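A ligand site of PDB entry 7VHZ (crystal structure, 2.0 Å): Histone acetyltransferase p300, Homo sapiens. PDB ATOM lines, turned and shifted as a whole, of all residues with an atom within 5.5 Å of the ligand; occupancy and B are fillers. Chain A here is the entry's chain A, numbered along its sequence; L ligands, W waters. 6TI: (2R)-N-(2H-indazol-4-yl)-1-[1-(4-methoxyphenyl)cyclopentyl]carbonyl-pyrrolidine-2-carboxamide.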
ATOM      1  N   PHE A 218       2.731  29.076 -15.612  1.00  0.00           N
ATOM      2  CA  PHE A 218       2.076  29.269 -14.325  1.00  0.00           C
ATOM      3  C   PHE A 218       2.144  30.731 -13.942  1.00  0.00           C
ATOM      4  O   PHE A 218       3.149  31.400 -14.186  1.00  0.00           O
ATOM      5  CB  PHE A 218       2.718  28.392 -13.232  1.00  0.00           C
ATOM      6  CG  PHE A 218       2.129  28.606 -11.859  1.00  0.00           C
ATOM      7  CD1 PHE A 218       1.020  27.896 -11.442  1.00  0.00           C
ATOM      8  CD2 PHE A 218       2.687  29.539 -10.990  1.00  0.00           C
ATOM      9  CE1 PHE A 218       0.493  28.085 -10.196  1.00  0.00           C
ATOM     10  CE2 PHE A 218       2.147  29.740  -9.742  1.00  0.00           C
ATOM     11  CZ  PHE A 218       1.046  29.015  -9.340  1.00  0.00           C
ATOM     12  N   LEU A 242      -4.738  32.251  -9.273  1.00  0.00           N
ATOM     13  CA  LEU A 242      -3.712  31.382  -9.817  1.00  0.00           C
ATOM     14  C   LEU A 242      -4.219  30.836 -11.141  1.00  0.00           C
ATOM     15  O   LEU A 242      -5.428  30.626 -11.307  1.00  0.00           O
ATOM     16  CB  LEU A 242      -3.331  30.244  -8.850  1.00  0.00           C
ATOM     17  CG  LEU A 242      -4.361  29.185  -8.448  1.00  0.00           C
ATOM     18  CD1 LEU A 242      -3.703  28.114  -7.604  1.00  0.00           C
ATOM     19  CD2 LEU A 242      -5.535  29.784  -7.678  1.00  0.00           C
ATOM     20  N   ASP A 243      -3.316  30.620 -12.084  1.00  0.00           N
ATOM     21  CA  ASP A 243      -3.698  30.176 -13.425  1.00  0.00           C
ATOM     22  C   ASP A 243      -2.554  29.385 -14.039  1.00  0.00           C
ATOM     23  O   ASP A 243      -1.418  29.437 -13.569  1.00  0.00           O
ATOM     24  CB  ASP A 243      -4.071  31.362 -14.320  1.00  0.00           C
ATOM     25  CG  ASP A 243      -5.008  30.971 -15.442  1.00  0.00           C
ATOM     26  OD1 ASP A 243      -5.456  29.805 -15.481  1.00  0.00           O
ATOM     27  OD2 ASP A 243      -5.302  31.845 -16.282  1.00  0.00           O
ATOM     28  N   SER A 244      -2.864  28.644 -15.102  1.00  0.00           N
ATOM     29  CA  SER A 244      -1.880  27.790 -15.733  1.00  0.00           C
ATOM     30  C   SER A 244      -2.243  27.581 -17.204  1.00  0.00           C
ATOM     31  O   SER A 244      -3.391  27.733 -17.614  1.00  0.00           O
ATOM     32  CB  SER A 244      -1.771  26.432 -15.023  1.00  0.00           C
ATOM     33  OG  SER A 244      -2.847  25.586 -15.394  1.00  0.00           O
ATOM     34  N   TYR A 258       3.392  22.489  -9.861  1.00  0.00           N
ATOM     35  CA  TYR A 258       2.494  23.484  -9.262  1.00  0.00           C
ATOM     36  C   TYR A 258       2.542  23.412  -7.747  1.00  0.00           C
ATOM     37  O   TYR A 258       2.645  24.435  -7.071  1.00  0.00           O
ATOM     38  CB  TYR A 258       1.050  23.260  -9.738  1.00  0.00           C
ATOM     39  CG  TYR A 258       0.816  23.361 -11.227  1.00  0.00           C
ATOM     40  CD1 TYR A 258       1.571  24.224 -12.006  1.00  0.00           C
ATOM     41  CD2 TYR A 258      -0.166  22.598 -11.846  1.00  0.00           C
ATOM     42  CE1 TYR A 258       1.359  24.332 -13.365  1.00  0.00           C
ATOM     43  CE2 TYR A 258      -0.392  22.700 -13.214  1.00  0.00           C
ATOM     44  CZ  TYR A 258       0.374  23.577 -13.961  1.00  0.00           C
ATOM     45  OH  TYR A 258       0.157  23.669 -15.315  1.00  0.00           O
ATOM     46  N   CYS A 282     -12.023  28.360  -5.300  1.00  0.00           N
ATOM     47  CA  CYS A 282     -13.200  28.553  -6.134  1.00  0.00           C
ATOM     48  C   CYS A 282     -12.727  28.630  -7.582  1.00  0.00           C
ATOM     49  O   CYS A 282     -11.916  29.520  -7.916  1.00  0.00           O
ATOM     50  CB  CYS A 282     -13.979  29.803  -5.756  1.00  0.00           C
ATOM     51  SG  CYS A 282     -15.504  29.993  -6.695  1.00  0.00           S
ATOM     52  N   PRO A 283     -13.167  27.724  -8.448  1.00  0.00           N
ATOM     53  CA  PRO A 283     -12.785  27.830  -9.859  1.00  0.00           C
ATOM     54  C   PRO A 283     -13.356  29.091 -10.477  1.00  0.00           C
ATOM     55  O   PRO A 283     -14.425  29.578 -10.063  1.00  0.00           O
ATOM     56  CB  PRO A 283     -13.394  26.574 -10.489  1.00  0.00           C
ATOM     57  CG  PRO A 283     -13.899  25.729  -9.338  1.00  0.00           C
ATOM     58  CD  PRO A 283     -14.149  26.660  -8.218  1.00  0.00           C
ATOM     59  N   PRO A 284     -12.664  29.661 -11.460  1.00  0.00           N
ATOM     60  CA  PRO A 284     -13.221  30.812 -12.183  1.00  0.00           C
ATOM     61  C   PRO A 284     -14.411  30.391 -13.030  1.00  0.00           C
ATOM     62  O   PRO A 284     -14.617  29.215 -13.339  1.00  0.00           O
ATOM     63  CB  PRO A 284     -12.060  31.281 -13.046  1.00  0.00           C
ATOM     64  CG  PRO A 284     -11.259  30.036 -13.295  1.00  0.00           C
ATOM     65  CD  PRO A 284     -11.383  29.236 -12.016  1.00  0.00           C
ATOM     66  N   SER A 285     -15.193  31.393 -13.432  1.00  0.00           N
ATOM     67  CA  SER A 285     -16.327  31.149 -14.309  1.00  0.00           C
ATOM     68  C   SER A 285     -15.857  30.614 -15.649  1.00  0.00           C
ATOM     69  O   SER A 285     -14.728  30.867 -16.096  1.00  0.00           O
ATOM     70  CB  SER A 285     -17.135  32.430 -14.514  1.00  0.00           C
ATOM     71  OG  SER A 285     -16.463  33.309 -15.396  1.00  0.00           O
ATOM     72  N   GLY A 287     -14.981  30.082 -19.339  1.00  0.00           N
ATOM     73  CA  GLY A 287     -14.435  31.070 -20.243  1.00  0.00           C
ATOM     74  C   GLY A 287     -13.025  30.688 -20.610  1.00  0.00           C
ATOM     75  O   GLY A 287     -12.489  29.671 -20.165  1.00  0.00           O
ATOM     76  N   ASP A 288     -12.406  31.536 -21.426  1.00  0.00           N
ATOM     77  CA  ASP A 288     -11.076  31.250 -21.923  1.00  0.00           C
ATOM     78  C   ASP A 288     -10.009  32.193 -21.392  1.00  0.00           C
ATOM     79  O   ASP A 288      -8.822  31.983 -21.689  1.00  0.00           O
ATOM     80  CB  ASP A 288     -11.077  31.282 -23.455  1.00  0.00           C
ATOM     81  CG  ASP A 288     -11.860  30.133 -24.066  1.00  0.00           C
ATOM     82  OD1 ASP A 288     -13.074  30.293 -24.290  1.00  0.00           O
ATOM     83  OD2 ASP A 288     -11.254  29.068 -24.326  1.00  0.00           O
ATOM     84  N   ASP A 289     -10.363  33.198 -20.597  1.00  0.00           N
ATOM     85  CA  ASP A 289      -9.411  34.179 -20.077  1.00  0.00           C
ATOM     86  C   ASP A 289      -9.528  34.237 -18.558  1.00  0.00           C
ATOM     87  O   ASP A 289     -10.626  34.483 -18.041  1.00  0.00           O
ATOM     88  CB  ASP A 289      -9.685  35.569 -20.660  1.00  0.00           C
ATOM     89  CG  ASP A 289      -9.591  35.609 -22.177  1.00  0.00           C
ATOM     90  OD1 ASP A 289      -9.172  34.619 -22.792  1.00  0.00           O
ATOM     91  OD2 ASP A 289      -9.937  36.667 -22.751  1.00  0.00           O
ATOM     92  N   TYR A 290      -8.424  33.980 -17.851  1.00  0.00           N
ATOM     93  CA  TYR A 290      -8.384  34.325 -16.426  1.00  0.00           C
ATOM     94  C   TYR A 290      -7.177  35.187 -16.055  1.00  0.00           C
ATOM     95  O   TYR A 290      -7.316  36.389 -15.804  1.00  0.00           O
ATOM     96  CB  TYR A 290      -8.363  33.033 -15.626  1.00  0.00           C
ATOM     97  CG  TYR A 290      -8.631  33.160 -14.157  1.00  0.00           C
ATOM     98  CD1 TYR A 290      -9.549  34.085 -13.667  1.00  0.00           C
ATOM     99  CD2 TYR A 290      -7.970  32.326 -13.251  1.00  0.00           C
ATOM    100  CE1 TYR A 290      -9.799  34.175 -12.306  1.00  0.00           C
ATOM    101  CE2 TYR A 290      -8.211  32.411 -11.899  1.00  0.00           C
ATOM    102  CZ  TYR A 290      -9.126  33.327 -11.432  1.00  0.00           C
ATOM    103  OH  TYR A 290      -9.333  33.378 -10.070  1.00  0.00           O
ATOM    104  N   HIS A 295      -7.048  30.120 -23.222  1.00  0.00           N
ATOM    105  CA  HIS A 295      -6.527  28.835 -22.757  1.00  0.00           C
ATOM    106  C   HIS A 295      -6.703  27.762 -23.828  1.00  0.00           C
ATOM    107  O   HIS A 295      -7.562  27.886 -24.716  1.00  0.00           O
ATOM    108  CB  HIS A 295      -7.249  28.406 -21.484  1.00  0.00           C
ATOM    109  CG  HIS A 295      -6.766  29.084 -20.242  1.00  0.00           C
ATOM    110  ND1 HIS A 295      -7.150  30.358 -19.897  1.00  0.00           N
ATOM    111  CD2 HIS A 295      -5.929  28.666 -19.264  1.00  0.00           C
ATOM    112  CE1 HIS A 295      -6.573  30.697 -18.756  1.00  0.00           C
ATOM    113  NE2 HIS A 295      -5.822  29.694 -18.350  1.00  0.00           N
ATOM    114  N   PRO A 296      -5.913  26.688 -23.778  1.00  0.00           N
ATOM    115  CA  PRO A 296      -6.113  25.577 -24.722  1.00  0.00           C
ATOM    116  C   PRO A 296      -7.512  25.004 -24.580  1.00  0.00           C
ATOM    117  O   PRO A 296      -8.013  24.824 -23.456  1.00  0.00           O
ATOM    118  CB  PRO A 296      -5.045  24.552 -24.295  1.00  0.00           C
ATOM    119  CG  PRO A 296      -4.031  25.348 -23.533  1.00  0.00           C
ATOM    120  CD  PRO A 296      -4.802  26.434 -22.850  1.00  0.00           C
ATOM    121  N   GLN A 299      -7.845  22.127 -22.214  1.00  0.00           N
ATOM    122  CA  GLN A 299      -7.589  22.385 -20.806  1.00  0.00           C
ATOM    123  C   GLN A 299      -8.893  22.844 -20.156  1.00  0.00           C
ATOM    124  O   GLN A 299      -9.449  23.877 -20.536  1.00  0.00           O
ATOM    125  CB  GLN A 299      -6.504  23.445 -20.603  1.00  0.00           C
ATOM    126  CG  GLN A 299      -6.107  23.625 -19.147  1.00  0.00           C
ATOM    127  CD  GLN A 299      -4.997  24.654 -18.954  1.00  0.00           C
ATOM    128  OE1 GLN A 299      -4.347  25.074 -19.911  1.00  0.00           O
ATOM    129  NE2 GLN A 299      -4.777  25.040 -17.708  1.00  0.00           N
ATOM    130  N   LYS A 300      -9.395  22.051 -19.220  1.00  0.00           N
ATOM    131  CA  LYS A 300     -10.686  22.297 -18.582  1.00  0.00           C
ATOM    132  C   LYS A 300     -10.505  22.930 -17.213  1.00  0.00           C
ATOM    133  O   LYS A 300      -9.543  22.608 -16.507  1.00  0.00           O
ATOM    134  CB  LYS A 300     -11.479  20.995 -18.465  1.00  0.00           C
ATOM    135  CG  LYS A 300     -11.641  20.253 -19.801  1.00  0.00           C
ATOM    136  CD  LYS A 300     -12.298  21.154 -20.840  1.00  0.00           C
ATOM    137  CE  LYS A 300     -12.486  20.434 -22.171  1.00  0.00           C
ATOM    138  NZ  LYS A 300     -13.287  21.250 -23.127  1.00  0.00           N
ATOM    139  N   ILE A 301     -11.402  23.839 -16.860  1.00  0.00           N
ATOM    140  CA  ILE A 301     -11.445  24.376 -15.492  1.00  0.00           C
ATOM    141  C   ILE A 301     -11.909  23.269 -14.546  1.00  0.00           C
ATOM    142  O   ILE A 301     -12.943  22.625 -14.808  1.00  0.00           O
ATOM    143  CB  ILE A 301     -12.387  25.580 -15.435  1.00  0.00           C
ATOM    144  CG1 ILE A 301     -11.866  26.711 -16.315  1.00  0.00           C
ATOM    145  CG2 ILE A 301     -12.556  26.057 -14.005  1.00  0.00           C
ATOM    146  CD1 ILE A 301     -12.841  27.904 -16.413  1.00  0.00           C
ATOM    147  N   PRO A 302     -11.193  22.998 -13.455  1.00  0.00           N
ATOM    148  CA  PRO A 302     -11.645  21.968 -12.515  1.00  0.00           C
ATOM    149  C   PRO A 302     -12.966  22.355 -11.866  1.00  0.00           C
ATOM    150  O   PRO A 302     -13.223  23.524 -11.594  1.00  0.00           O
ATOM    151  CB  PRO A 302     -10.514  21.909 -11.484  1.00  0.00           C
ATOM    152  CG  PRO A 302      -9.886  23.295 -11.548  1.00  0.00           C
ATOM    153  CD  PRO A 302      -9.969  23.667 -13.001  1.00  0.00           C
ATOM    154  N   ARG A 306     -12.993  18.846  -7.154  1.00  0.00           N
ATOM    155  CA  ARG A 306     -11.662  18.420  -7.574  1.00  0.00           C
ATOM    156  C   ARG A 306     -10.615  19.479  -7.278  1.00  0.00           C
ATOM    157  O   ARG A 306      -9.476  19.155  -6.934  1.00  0.00           O
ATOM    158  CB  ARG A 306     -11.684  18.029  -9.058  1.00  0.00           C
ATOM    159  CG  ARG A 306     -12.339  16.649  -9.279  1.00  0.00           C
ATOM    160  CD  ARG A 306     -12.158  16.127 -10.681  1.00  0.00           C
ATOM    161  NE  ARG A 306     -10.792  15.657 -10.919  1.00  0.00           N
ATOM    162  CZ  ARG A 306      -9.969  16.187 -11.805  1.00  0.00           C
ATOM    163  NH1 ARG A 306     -10.336  17.203 -12.578  1.00  0.00           N
ATOM    164  NH2 ARG A 306      -8.740  15.681 -11.942  1.00  0.00           N
ATOM    165  N   LEU A 307     -10.966  20.760  -7.436  1.00  0.00           N
ATOM    166  CA  LEU A 307     -10.037  21.823  -7.049  1.00  0.00           C
ATOM    167  C   LEU A 307      -9.746  21.784  -5.550  1.00  0.00           C
ATOM    168  O   LEU A 307      -8.597  21.959  -5.135  1.00  0.00           O
ATOM    169  CB  LEU A 307     -10.597  23.193  -7.456  1.00  0.00           C
ATOM    170  CG  LEU A 307      -9.670  24.384  -7.182  1.00  0.00           C
ATOM    171  CD1 LEU A 307      -8.298  24.179  -7.868  1.00  0.00           C
ATOM    172  CD2 LEU A 307     -10.306  25.704  -7.633  1.00  0.00           C
ATOM    173  N   TRP A 310      -7.399  19.005  -4.877  1.00  0.00           N
ATOM    174  CA  TRP A 310      -6.077  19.394  -5.344  1.00  0.00           C
ATOM    175  C   TRP A 310      -5.364  20.244  -4.299  1.00  0.00           C
ATOM    176  O   TRP A 310      -4.174  20.017  -4.012  1.00  0.00           O
ATOM    177  CB  TRP A 310      -6.221  20.147  -6.673  1.00  0.00           C
ATOM    178  CG  TRP A 310      -4.957  20.491  -7.401  1.00  0.00           C
ATOM    179  CD1 TRP A 310      -4.328  19.734  -8.350  1.00  0.00           C
ATOM    180  CD2 TRP A 310      -4.205  21.703  -7.281  1.00  0.00           C
ATOM    181  NE1 TRP A 310      -3.218  20.395  -8.819  1.00  0.00           N
ATOM    182  CE2 TRP A 310      -3.122  21.604  -8.181  1.00  0.00           C
ATOM    183  CE3 TRP A 310      -4.330  22.849  -6.497  1.00  0.00           C
ATOM    184  CZ2 TRP A 310      -2.174  22.624  -8.310  1.00  0.00           C
ATOM    185  CZ3 TRP A 310      -3.379  23.855  -6.624  1.00  0.00           C
ATOM    186  CH2 TRP A 310      -2.315  23.736  -7.528  1.00  0.00           C
HETATM  187  N   6TI L   1      -6.404  26.491 -12.137  1.00  0.00           N
HETATM  188  CA  6TI L   1      -6.911  27.499 -13.079  1.00  0.00           C
HETATM  189  C   6TI L   1      -7.488  26.984 -14.267  1.00  0.00           C
HETATM  190  O   6TI L   1      -7.830  25.811 -14.322  1.00  0.00           O
HETATM  191  CB  6TI L   1      -7.927  28.187 -12.259  1.00  0.00           C
HETATM  192  CG  6TI L   1      -8.563  27.128 -11.420  1.00  0.00           C
HETATM  193  CD  6TI L   1      -7.392  26.347 -11.002  1.00  0.00           C
HETATM  194  CAA 6TI L   1      -5.218  25.946 -12.443  1.00  0.00           C
HETATM  195  CAI 6TI L   1      -8.174  27.626 -16.452  1.00  0.00           C
HETATM  196  CAJ 6TI L   1      -8.075  26.460 -17.206  1.00  0.00           C
HETATM  197  CAK 6TI L   1      -8.729  26.387 -18.424  1.00  0.00           C
HETATM  198  CAL 6TI L   1      -9.454  27.476 -18.851  1.00  0.00           C
HETATM  199  CAM 6TI L   1      -9.502  28.567 -18.100  1.00  0.00           C
HETATM  200  CAN 6TI L   1      -8.873  28.634 -16.941  1.00  0.00           C
HETATM  201  CAO 6TI L   1      -9.158  29.829 -16.493  1.00  0.00           C
HETATM  202  CAT 6TI L   1      -4.608  24.861 -11.539  1.00  0.00           C
HETATM  203  CAU 6TI L   1      -5.359  23.688 -11.505  1.00  0.00           C
HETATM  204  CAV 6TI L   1      -5.756  23.107 -12.701  1.00  0.00           C
HETATM  205  CAW 6TI L   1      -6.498  21.933 -12.702  1.00  0.00           C
HETATM  206  CAX 6TI L   1      -6.845  21.331 -11.512  1.00  0.00           C
HETATM  207  CAY 6TI L   1      -6.448  21.912 -10.316  1.00  0.00           C
HETATM  208  CAZ 6TI L   1      -5.705  23.087 -10.316  1.00  0.00           C
HETATM  209  CBB 6TI L   1      -7.701  19.610 -10.247  1.00  0.00           C
HETATM  210  CBC 6TI L   1      -3.270  24.498 -12.084  1.00  0.00           C
HETATM  211  CBD 6TI L   1      -2.262  25.376 -11.369  1.00  0.00           C
HETATM  212  CBE 6TI L   1      -3.059  26.231 -10.492  1.00  0.00           C
HETATM  213  CBF 6TI L   1      -4.241  25.363 -10.174  1.00  0.00           C
HETATM  214  NAH 6TI L   1      -7.603  27.886 -15.268  1.00  0.00           N
HETATM  215  NAP 6TI L   1      -9.920  30.409 -17.412  1.00  0.00           N
HETATM  216  NAQ 6TI L   1     -10.099  29.736 -18.269  1.00  0.00           N
HETATM  217  OAS 6TI L   1      -4.627  26.276 -13.458  1.00  0.00           O
HETATM  218  OBA 6TI L   1      -7.569  20.183 -11.533  1.00  0.00           O
HETATM  219  O   HOH W   1      -7.081  23.625 -15.719  1.00  0.00           O
HETATM  220  O   HOH W   2     -12.439  32.141 -16.623  1.00  0.00           O
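Water W1 lies within hydrogen-bond range of an oxygen (O) of the ligand (2.7 Å), the backbone carbonyl oxygen of Lys 300 (2.8 Å) and the side-chain amide nitrogen of Gln 299 (3.4 Å). Water W2 lies within hydrogen-bond range of O of Ser 285 (2.7 Å), NAP of the ligand (3.2 Å) and O of Asp 289 (3.3 Å).
NE2 of His 295 is in hydrogen-bond range of OD1 of Asp 243 (2.9 Å). A ring nitrogen (ND1) of His 295 is in hydrogen-bond range of the backbone carbonyl oxygen (O) of Asp 288 (2.9 Å). The backbone carbonyl oxygen (O) of Ser 244 lies close to a ring nitrogen (NE2) of His 295 (3.2 Å). The backbone carbonyl oxygen (O) of Ser 244 is in hydrogen-bond range of the side-chain amide nitrogen (NE2) of Gln 299, 3.0 Å away.
Leu 242 touches the ligand (CD1 to CBE, 3.5 Å). Tyr 258 touches the ligand (CD2 to CBD, 3.5 Å). Pro 284 touches the ligand (CD to CG, 3.6 Å). C of Asp 288 touches NAQ of the ligand (3.97 Å). Tyr 290 touches the ligand. Gln 299 touches the ligand. CG1 of Ile 301 touches CAM of the ligand, 3.5 Å away. Pro 302 touches the ligand (CD to O, 3.3 Å). Arg 306 touches the ligand. CD1 of Leu 307 touches CAZ of the ligand, at 3.7 Å. Trp 310 touches the ligand. The nearest printed residue that does not touch the ligand is Asp 289 (4.02 Å).
The side-chain hydroxyl of Ser 244 sits at hydrogen-bond distance from an oxygen (OAS) of the ligand. The side-chain carboxylate of Asp 243 is in hydrogen-bond range of a nitrogen (NAH) of the ligand. NAQ of the ligand sits at hydrogen-bond distance from O of Gly 287. The backbone NH of Ser 244 lies close to an oxygen (OAS) of the ligand, at 3.4 Å. A ring nitrogen (ND1) of His 295 is in hydrogen-bond range of a nitrogen (NAQ) of the ligand, at 3.4 Å.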
